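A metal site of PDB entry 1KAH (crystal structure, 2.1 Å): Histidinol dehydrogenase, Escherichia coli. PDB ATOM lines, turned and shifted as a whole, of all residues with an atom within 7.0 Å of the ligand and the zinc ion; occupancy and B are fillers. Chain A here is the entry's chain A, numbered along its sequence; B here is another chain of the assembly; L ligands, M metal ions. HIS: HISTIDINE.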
ATOM      1  N   LEU A 138      -3.414 -17.216  19.720  1.00  0.00           N
ATOM      2  CA  LEU A 138      -3.863 -17.932  20.903  1.00  0.00           C
ATOM      3  C   LEU A 138      -3.233 -19.319  20.907  1.00  0.00           C
ATOM      4  O   LEU A 138      -3.915 -20.337  20.745  1.00  0.00           O
ATOM      5  CB  LEU A 138      -5.397 -18.026  20.935  1.00  0.00           C
ATOM      6  CG  LEU A 138      -6.127 -16.705  21.225  1.00  0.00           C
ATOM      7  CD1 LEU A 138      -6.081 -15.801  20.011  1.00  0.00           C
ATOM      8  CD2 LEU A 138      -7.576 -16.973  21.587  1.00  0.00           C
ATOM      9  N   SER A 140      -2.513 -21.204  23.045  1.00  0.00           N
ATOM     10  CA  SER A 140      -3.049 -22.131  24.034  1.00  0.00           C
ATOM     11  C   SER A 140      -3.831 -23.265  23.368  1.00  0.00           C
ATOM     12  O   SER A 140      -3.830 -24.387  23.854  1.00  0.00           O
ATOM     13  CB  SER A 140      -3.937 -21.401  25.044  1.00  0.00           C
ATOM     14  OG  SER A 140      -4.944 -20.637  24.401  1.00  0.00           O
ATOM     15  N   THR A 141      -4.497 -22.944  22.260  1.00  0.00           N
ATOM     16  CA  THR A 141      -5.278 -23.926  21.518  1.00  0.00           C
ATOM     17  C   THR A 141      -4.378 -25.081  21.045  1.00  0.00           C
ATOM     18  O   THR A 141      -4.844 -26.219  20.895  1.00  0.00           O
ATOM     19  CB  THR A 141      -5.939 -23.279  20.293  1.00  0.00           C
ATOM     20  OG1 THR A 141      -6.848 -22.255  20.731  1.00  0.00           O
ATOM     21  CG2 THR A 141      -6.708 -24.311  19.494  1.00  0.00           C
ATOM     22  N   PRO A 236     -20.505 -18.703  17.666  1.00  0.00           N
ATOM     23  CA  PRO A 236     -19.951 -17.653  18.529  1.00  0.00           C
ATOM     24  C   PRO A 236     -19.760 -18.220  19.938  1.00  0.00           C
ATOM     25  O   PRO A 236     -20.572 -19.025  20.392  1.00  0.00           O
ATOM     26  CB  PRO A 236     -21.029 -16.567  18.509  1.00  0.00           C
ATOM     27  CG  PRO A 236     -21.771 -16.824  17.205  1.00  0.00           C
ATOM     28  CD  PRO A 236     -21.845 -18.321  17.165  1.00  0.00           C
ATOM     29  N   SER A 237     -18.716 -17.785  20.646  1.00  0.00           N
ATOM     30  CA  SER A 237     -18.482 -18.272  21.997  1.00  0.00           C
ATOM     31  C   SER A 237     -19.563 -17.757  22.949  1.00  0.00           C
ATOM     32  O   SER A 237     -20.208 -16.754  22.649  1.00  0.00           O
ATOM     33  CB  SER A 237     -17.108 -17.806  22.470  1.00  0.00           C
ATOM     34  OG  SER A 237     -16.130 -18.289  21.581  1.00  0.00           O
ATOM     35  N   GLU A 238     -19.755 -18.424  24.082  1.00  0.00           N
ATOM     36  CA  GLU A 238     -20.779 -17.985  25.036  1.00  0.00           C
ATOM     37  C   GLU A 238     -20.357 -18.155  26.481  1.00  0.00           C
ATOM     38  O   GLU A 238     -19.592 -19.055  26.832  1.00  0.00           O
ATOM     39  CB  GLU A 238     -22.078 -18.784  24.832  1.00  0.00           C
ATOM     40  CG  GLU A 238     -22.412 -19.180  23.415  1.00  0.00           C
ATOM     41  CD  GLU A 238     -23.534 -20.217  23.343  1.00  0.00           C
ATOM     42  OE1 GLU A 238     -23.573 -21.126  24.210  1.00  0.00           O
ATOM     43  OE2 GLU A 238     -24.371 -20.136  22.418  1.00  0.00           O
ATOM     44  N   SER A 258     -14.067 -11.283  30.183  1.00  0.00           N
ATOM     45  CA  SER A 258     -13.107 -12.259  29.660  1.00  0.00           C
ATOM     46  C   SER A 258     -13.687 -12.844  28.382  1.00  0.00           C
ATOM     47  O   SER A 258     -13.013 -12.971  27.369  1.00  0.00           O
ATOM     48  CB  SER A 258     -12.883 -13.396  30.650  1.00  0.00           C
ATOM     49  OG  SER A 258     -12.037 -13.007  31.710  1.00  0.00           O
ATOM     50  N   GLN A 259     -14.955 -13.239  28.458  1.00  0.00           N
ATOM     51  CA  GLN A 259     -15.627 -13.825  27.315  1.00  0.00           C
ATOM     52  C   GLN A 259     -15.846 -12.766  26.223  1.00  0.00           C
ATOM     53  O   GLN A 259     -15.597 -13.020  25.049  1.00  0.00           O
ATOM     54  CB  GLN A 259     -16.965 -14.390  27.746  1.00  0.00           C
ATOM     55  CG  GLN A 259     -17.738 -15.030  26.627  1.00  0.00           C
ATOM     56  CD  GLN A 259     -16.974 -16.160  25.986  1.00  0.00           C
ATOM     57  OE1 GLN A 259     -16.529 -16.052  24.837  1.00  0.00           O
ATOM     58  NE2 GLN A 259     -16.801 -17.246  26.717  1.00  0.00           N
ATOM     59  N   GLU A 261     -14.198 -10.005  25.572  1.00  0.00           N
ATOM     60  CA  GLU A 261     -12.975  -9.556  24.905  1.00  0.00           C
ATOM     61  C   GLU A 261     -12.486 -10.474  23.792  1.00  0.00           C
ATOM     62  O   GLU A 261     -11.554 -10.119  23.049  1.00  0.00           O
ATOM     63  CB  GLU A 261     -11.848  -9.339  25.934  1.00  0.00           C
ATOM     64  CG  GLU A 261     -10.940 -10.534  26.184  1.00  0.00           C
ATOM     65  CD  GLU A 261      -9.727 -10.164  27.048  1.00  0.00           C
ATOM     66  OE1 GLU A 261      -9.383  -8.965  27.077  1.00  0.00           O
ATOM     67  OE2 GLU A 261      -9.124 -11.059  27.680  1.00  0.00           O
ATOM     68  N   HIS A 262     -13.087 -11.654  23.654  1.00  0.00           N
ATOM     69  CA  HIS A 262     -12.683 -12.553  22.573  1.00  0.00           C
ATOM     70  C   HIS A 262     -13.081 -11.946  21.223  1.00  0.00           C
ATOM     71  O   HIS A 262     -12.227 -11.552  20.443  1.00  0.00           O
ATOM     72  CB  HIS A 262     -13.340 -13.934  22.718  1.00  0.00           C
ATOM     73  CG  HIS A 262     -12.579 -14.875  23.605  1.00  0.00           C
ATOM     74  ND1 HIS A 262     -11.220 -15.091  23.470  1.00  0.00           N
ATOM     75  CD2 HIS A 262     -12.992 -15.658  24.630  1.00  0.00           C
ATOM     76  CE1 HIS A 262     -10.832 -15.979  24.370  1.00  0.00           C
ATOM     77  NE2 HIS A 262     -11.890 -16.331  25.090  1.00  0.00           N
ATOM     78  N   GLU A 326     -22.021 -22.504  26.410  1.00  0.00           N
ATOM     79  CA  GLU A 326     -20.724 -23.123  26.188  1.00  0.00           C
ATOM     80  C   GLU A 326     -19.952 -23.193  27.516  1.00  0.00           C
ATOM     81  O   GLU A 326     -19.365 -24.223  27.856  1.00  0.00           O
ATOM     82  CB  GLU A 326     -19.928 -22.318  25.171  1.00  0.00           C
ATOM     83  CG  GLU A 326     -18.563 -22.902  24.866  1.00  0.00           C
ATOM     84  CD  GLU A 326     -17.707 -21.944  24.077  1.00  0.00           C
ATOM     85  OE1 GLU A 326     -18.033 -20.742  24.031  1.00  0.00           O
ATOM     86  OE2 GLU A 326     -16.672 -22.388  23.531  1.00  0.00           O
ATOM     87  N   HIS A 327     -19.940 -22.078  28.245  1.00  0.00           N
ATOM     88  CA  HIS A 327     -19.272 -22.006  29.542  1.00  0.00           C
ATOM     89  C   HIS A 327     -20.328 -21.578  30.550  1.00  0.00           C
ATOM     90  O   HIS A 327     -21.024 -20.594  30.327  1.00  0.00           O
ATOM     91  CB  HIS A 327     -18.172 -20.948  29.594  1.00  0.00           C
ATOM     92  CG  HIS A 327     -17.156 -21.049  28.508  1.00  0.00           C
ATOM     93  ND1 HIS A 327     -17.303 -20.404  27.293  1.00  0.00           N
ATOM     94  CD2 HIS A 327     -15.946 -21.652  28.472  1.00  0.00           C
ATOM     95  CE1 HIS A 327     -16.228 -20.608  26.561  1.00  0.00           C
ATOM     96  NE2 HIS A 327     -15.385 -21.355  27.248  1.00  0.00           N
ATOM     97  N   GLU A 356     -13.064 -18.312  34.291  1.00  0.00           N
ATOM     98  CA  GLU A 356     -13.002 -18.944  32.983  1.00  0.00           C
ATOM     99  C   GLU A 356     -11.539 -19.037  32.522  1.00  0.00           C
ATOM    100  O   GLU A 356     -11.138 -20.017  31.881  1.00  0.00           O
ATOM    101  CB  GLU A 356     -13.806 -18.129  31.967  1.00  0.00           C
ATOM    102  CG  GLU A 356     -14.125 -18.918  30.712  1.00  0.00           C
ATOM    103  CD  GLU A 356     -14.279 -18.032  29.497  1.00  0.00           C
ATOM    104  OE1 GLU A 356     -13.265 -17.405  29.099  1.00  0.00           O
ATOM    105  OE2 GLU A 356     -15.411 -17.963  28.967  1.00  0.00           O
ATOM    106  N   SER A 357     -10.757 -18.018  32.848  1.00  0.00           N
ATOM    107  CA  SER A 357      -9.340 -17.930  32.487  1.00  0.00           C
ATOM    108  C   SER A 357      -8.568 -19.173  32.913  1.00  0.00           C
ATOM    109  O   SER A 357      -7.668 -19.621  32.207  1.00  0.00           O
ATOM    110  CB  SER A 357      -8.688 -16.723  33.151  1.00  0.00           C
ATOM    111  OG  SER A 357      -9.562 -15.627  33.183  1.00  0.00           O
ATOM    112  N   GLY A 359      -9.734 -22.267  33.195  1.00  0.00           N
ATOM    113  CA  GLY A 359     -10.072 -23.332  32.261  1.00  0.00           C
ATOM    114  C   GLY A 359      -9.500 -23.093  30.864  1.00  0.00           C
ATOM    115  O   GLY A 359      -9.104 -24.033  30.187  1.00  0.00           O
ATOM    116  N   ASP A 360      -9.467 -21.849  30.428  1.00  0.00           N
ATOM    117  CA  ASP A 360      -8.923 -21.581  29.105  1.00  0.00           C
ATOM    118  C   ASP A 360      -7.415 -21.874  29.088  1.00  0.00           C
ATOM    119  O   ASP A 360      -6.856 -22.178  28.045  1.00  0.00           O
ATOM    120  CB  ASP A 360      -9.138 -20.117  28.685  1.00  0.00           C
ATOM    121  CG  ASP A 360     -10.612 -19.738  28.612  1.00  0.00           C
ATOM    122  OD1 ASP A 360     -11.447 -20.633  28.385  1.00  0.00           O
ATOM    123  OD2 ASP A 360     -10.925 -18.536  28.753  1.00  0.00           O
ATOM    124  N   TYR A 361      -6.782 -21.822  30.260  1.00  0.00           N
ATOM    125  CA  TYR A 361      -5.338 -21.983  30.303  1.00  0.00           C
ATOM    126  C   TYR A 361      -4.638 -23.122  31.020  1.00  0.00           C
ATOM    127  O   TYR A 361      -3.794 -23.785  30.425  1.00  0.00           O
ATOM    128  CB  TYR A 361      -4.687 -20.683  30.810  1.00  0.00           C
ATOM    129  CG  TYR A 361      -4.875 -19.506  29.888  1.00  0.00           C
ATOM    130  CD1 TYR A 361      -5.637 -18.409  30.270  1.00  0.00           C
ATOM    131  CD2 TYR A 361      -4.297 -19.492  28.621  1.00  0.00           C
ATOM    132  CE1 TYR A 361      -5.840 -17.334  29.416  1.00  0.00           C
ATOM    133  CE2 TYR A 361      -4.480 -18.413  27.754  1.00  0.00           C
ATOM    134  CZ  TYR A 361      -5.249 -17.340  28.148  1.00  0.00           C
ATOM    135  OH  TYR A 361      -5.461 -16.285  27.297  1.00  0.00           O
ATOM    136  N   ASN A 366     -10.476 -28.977  28.735  1.00  0.00           N
ATOM    137  CA  ASN A 366     -10.251 -28.536  27.372  1.00  0.00           C
ATOM    138  C   ASN A 366     -11.126 -27.330  27.066  1.00  0.00           C
ATOM    139  O   ASN A 366     -12.326 -27.364  27.331  1.00  0.00           O
ATOM    140  CB  ASN A 366     -10.546 -29.659  26.382  1.00  0.00           C
ATOM    141  CG  ASN A 366      -9.731 -29.521  25.102  1.00  0.00           C
ATOM    142  OD1 ASN A 366      -9.967 -28.617  24.297  1.00  0.00           O
ATOM    143  ND2 ASN A 366      -8.772 -30.408  24.920  1.00  0.00           N
ATOM    144  N   HIS A 367     -10.539 -26.278  26.504  1.00  0.00           N
ATOM    145  CA  HIS A 367     -11.315 -25.087  26.199  1.00  0.00           C
ATOM    146  C   HIS A 367     -11.945 -25.115  24.816  1.00  0.00           C
ATOM    147  O   HIS A 367     -12.521 -24.139  24.361  1.00  0.00           O
ATOM    148  CB  HIS A 367     -10.478 -23.796  26.396  1.00  0.00           C
ATOM    149  CG  HIS A 367      -9.457 -23.534  25.331  1.00  0.00           C
ATOM    150  ND1 HIS A 367      -8.275 -22.866  25.592  1.00  0.00           N
ATOM    151  CD2 HIS A 367      -9.479 -23.722  23.984  1.00  0.00           C
ATOM    152  CE1 HIS A 367      -7.620 -22.662  24.455  1.00  0.00           C
ATOM    153  NE2 HIS A 367      -8.332 -23.164  23.467  1.00  0.00           N
ATOM    154  N   VAL A 368     -11.830 -26.263  24.153  1.00  0.00           N
ATOM    155  CA  VAL A 368     -12.440 -26.414  22.833  1.00  0.00           C
ATOM    156  C   VAL A 368     -13.755 -27.073  23.173  1.00  0.00           C
ATOM    157  O   VAL A 368     -13.831 -28.292  23.372  1.00  0.00           O
ATOM    158  CB  VAL A 368     -11.612 -27.321  21.906  1.00  0.00           C
ATOM    159  CG1 VAL A 368     -12.410 -27.585  20.619  1.00  0.00           C
ATOM    160  CG2 VAL A 368     -10.295 -26.642  21.575  1.00  0.00           C
ATOM    161  N   LEU A 369     -14.787 -26.254  23.225  1.00  0.00           N
ATOM    162  CA  LEU A 369     -16.108 -26.697  23.631  1.00  0.00           C
ATOM    163  C   LEU A 369     -17.202 -26.461  22.605  1.00  0.00           C
ATOM    164  O   LEU A 369     -17.060 -25.642  21.693  1.00  0.00           O
ATOM    165  CB  LEU A 369     -16.483 -25.965  24.920  1.00  0.00           C
ATOM    166  CG  LEU A 369     -15.457 -26.015  26.042  1.00  0.00           C
ATOM    167  CD1 LEU A 369     -15.717 -24.875  27.023  1.00  0.00           C
ATOM    168  CD2 LEU A 369     -15.527 -27.372  26.720  1.00  0.00           C
ATOM    169  N   ALA B 411      -2.163 -15.669  29.724  1.00  0.00           N
ATOM    170  CA  ALA B 411      -3.147 -14.701  29.270  1.00  0.00           C
ATOM    171  C   ALA B 411      -2.444 -13.477  28.714  1.00  0.00           C
ATOM    172  O   ALA B 411      -2.828 -12.948  27.660  1.00  0.00           O
ATOM    173  CB  ALA B 411      -4.046 -14.298  30.410  1.00  0.00           C
ATOM    174  N   GLU B 414      -1.019 -14.045  25.334  1.00  0.00           N
ATOM    175  CA  GLU B 414      -2.011 -14.034  24.257  1.00  0.00           C
ATOM    176  C   GLU B 414      -2.597 -12.640  24.082  1.00  0.00           C
ATOM    177  O   GLU B 414      -3.447 -12.424  23.221  1.00  0.00           O
ATOM    178  CB  GLU B 414      -3.139 -15.042  24.532  1.00  0.00           C
ATOM    179  CG  GLU B 414      -2.673 -16.481  24.704  1.00  0.00           C
ATOM    180  CD  GLU B 414      -3.803 -17.493  24.544  1.00  0.00           C
ATOM    181  OE1 GLU B 414      -4.885 -17.305  25.159  1.00  0.00           O
ATOM    182  OE2 GLU B 414      -3.612 -18.492  23.816  1.00  0.00           O
ATOM    183  N   LEU B 416      -4.574 -10.946  26.128  1.00  0.00           N
ATOM    184  CA  LEU B 416      -5.972 -10.937  26.531  1.00  0.00           C
ATOM    185  C   LEU B 416      -5.973 -10.413  27.957  1.00  0.00           C
ATOM    186  O   LEU B 416      -5.987 -11.187  28.926  1.00  0.00           O
ATOM    187  CB  LEU B 416      -6.559 -12.353  26.472  1.00  0.00           C
ATOM    188  CG  LEU B 416      -6.730 -12.946  25.062  1.00  0.00           C
ATOM    189  CD1 LEU B 416      -7.381 -14.299  25.152  1.00  0.00           C
ATOM    190  CD2 LEU B 416      -7.600 -12.007  24.201  1.00  0.00           C
ATOM    191  N   HIS B 419      -8.667 -11.462  30.579  1.00  0.00           N
ATOM    192  CA  HIS B 419      -8.474 -12.802  31.114  1.00  0.00           C
ATOM    193  C   HIS B 419      -7.483 -12.724  32.254  1.00  0.00           C
ATOM    194  O   HIS B 419      -7.612 -13.422  33.253  1.00  0.00           O
ATOM    195  CB  HIS B 419      -7.937 -13.759  30.053  1.00  0.00           C
ATOM    196  CG  HIS B 419      -8.968 -14.244  29.076  1.00  0.00           C
ATOM    197  ND1 HIS B 419      -9.607 -13.401  28.204  1.00  0.00           N
ATOM    198  CD2 HIS B 419      -9.459 -15.488  28.849  1.00  0.00           C
ATOM    199  CE1 HIS B 419     -10.440 -14.108  27.451  1.00  0.00           C
ATOM    200  NE2 HIS B 419     -10.375 -15.372  27.830  1.00  0.00           N
HETATM  201  N   HIS L   1     -12.543 -18.733  26.022  1.00  0.00           N
HETATM  202  CA  HIS L   1     -12.210 -19.365  24.707  1.00  0.00           C
HETATM  203  C   HIS L   1     -13.303 -20.354  24.275  1.00  0.00           C
HETATM  204  O   HIS L   1     -13.549 -21.322  25.024  1.00  0.00           O
HETATM  205  CB  HIS L   1     -10.860 -20.095  24.804  1.00  0.00           C
HETATM  206  CG  HIS L   1      -9.688 -19.198  25.071  1.00  0.00           C
HETATM  207  ND1 HIS L   1      -9.660 -18.299  26.131  1.00  0.00           N
HETATM  208  CD2 HIS L   1      -8.494 -19.070  24.450  1.00  0.00           C
HETATM  209  CE1 HIS L   1      -8.504 -17.671  26.133  1.00  0.00           C
HETATM  210  NE2 HIS L   1      -7.767 -18.115  25.121  1.00  0.00           N
HETATM  211  OXT HIS L   1     -13.897 -20.162  23.187  1.00  0.00           O
HETATM  212 ZN    ZN M   1     -11.076 -17.284  26.995  1.00  0.00          ZN
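OD2 of Asp 360 lies close to OE1 of Glu 356, at 2.6 Å. The backbone carbonyl oxygen (O) of His 419 of chain B lies within hydrogen-bond range of the side-chain hydroxyl (OG) of Ser 357, at 2.9 Å. A ring nitrogen (ND1) of His 419 of chain B sits at hydrogen-bond distance from the side-chain carboxylate of Glu 261, 2.4 Å away. The side-chain carboxylate of Glu 326 lies close to a ring nitrogen (ND1) of His 327. ND1 of His 327 sits at hydrogen-bond distance from NE2 of Gln 259 (3.2 Å). OE1 of Glu 414 of chain B sits at hydrogen-bond distance from OH of Tyr 361 (2.4 Å). The side-chain hydroxyl (OG1) of Thr 141 is in hydrogen-bond range of a ring nitrogen (NE2) of His 367, 3.2 Å away. N of Leu 416 of chain B sits at hydrogen-bond distance from O of Ala 411 of chain B, at 3.1 Å.
A ring nitrogen (NE2) of His 327 lies within hydrogen-bond range of an oxygen (O) of the ligand (2.9 Å). A nitrogen (NE2) of the ligand lies within hydrogen-bond range of the side-chain carboxylate of Glu 414 of chain B, at 3.0 Å. A nitrogen (N) of the ligand lies close to the side-chain carboxylate (OE1) of Glu 356, 3.4 Å away. O of His 367 lies close to O of the ligand. The side-chain hydroxyl (OG) of Ser 237 sits at hydrogen-bond distance from an oxygen (OXT) of the ligand (3.3 Å).
Glu 356 touches the zinc ion. Four residues have an atom within 4 Å of the zinc ion: His 262, Glu 356, Asp 360 and His 419 of chain B.
Leu 138 touches the ligand (CD2 to CD2, 3.7 Å). Ser 140 touches the ligand. Glu 326 touches the ligand. OH of Tyr 361 touches CE1 of the ligand, 3.5 Å away. Leu 416 of chain B touches the ligand (CD1 to CE1, 3.7 Å). Hydrophobic or aromatic side chains within 4 Å of the ligand: Leu 138, His 262, His 327, Tyr 361, His 367, Leu 416 of chain B and His 419 of chain B. 13 residues have an atom within 4 Å of the ligand: Leu 138, Ser 140, Ser 237, His 262, Glu 326, His 327, Glu 356, Asp 360, Tyr 361, His 367, Glu 414 of chain B, Leu 416 of chain B and His 419 of chain B. Along chain A the residues within 4 Å of the ligand span positions 138 to 367. The nearest printed residue that does not touch the ligand is Gln 259 (4.6 Å).
ND1 of the ligand binds the zinc ion (1.9 Å). The zinc ion is bound by OD2 of Asp 360 (2.2 Å). A ring nitrogen (NE2) of His 419 of chain B binds the zinc ion. The zinc ion is bound by N of the ligand, at 2.3 Å. A ring nitrogen (NE2) of His 262 is bound to the zinc ion.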
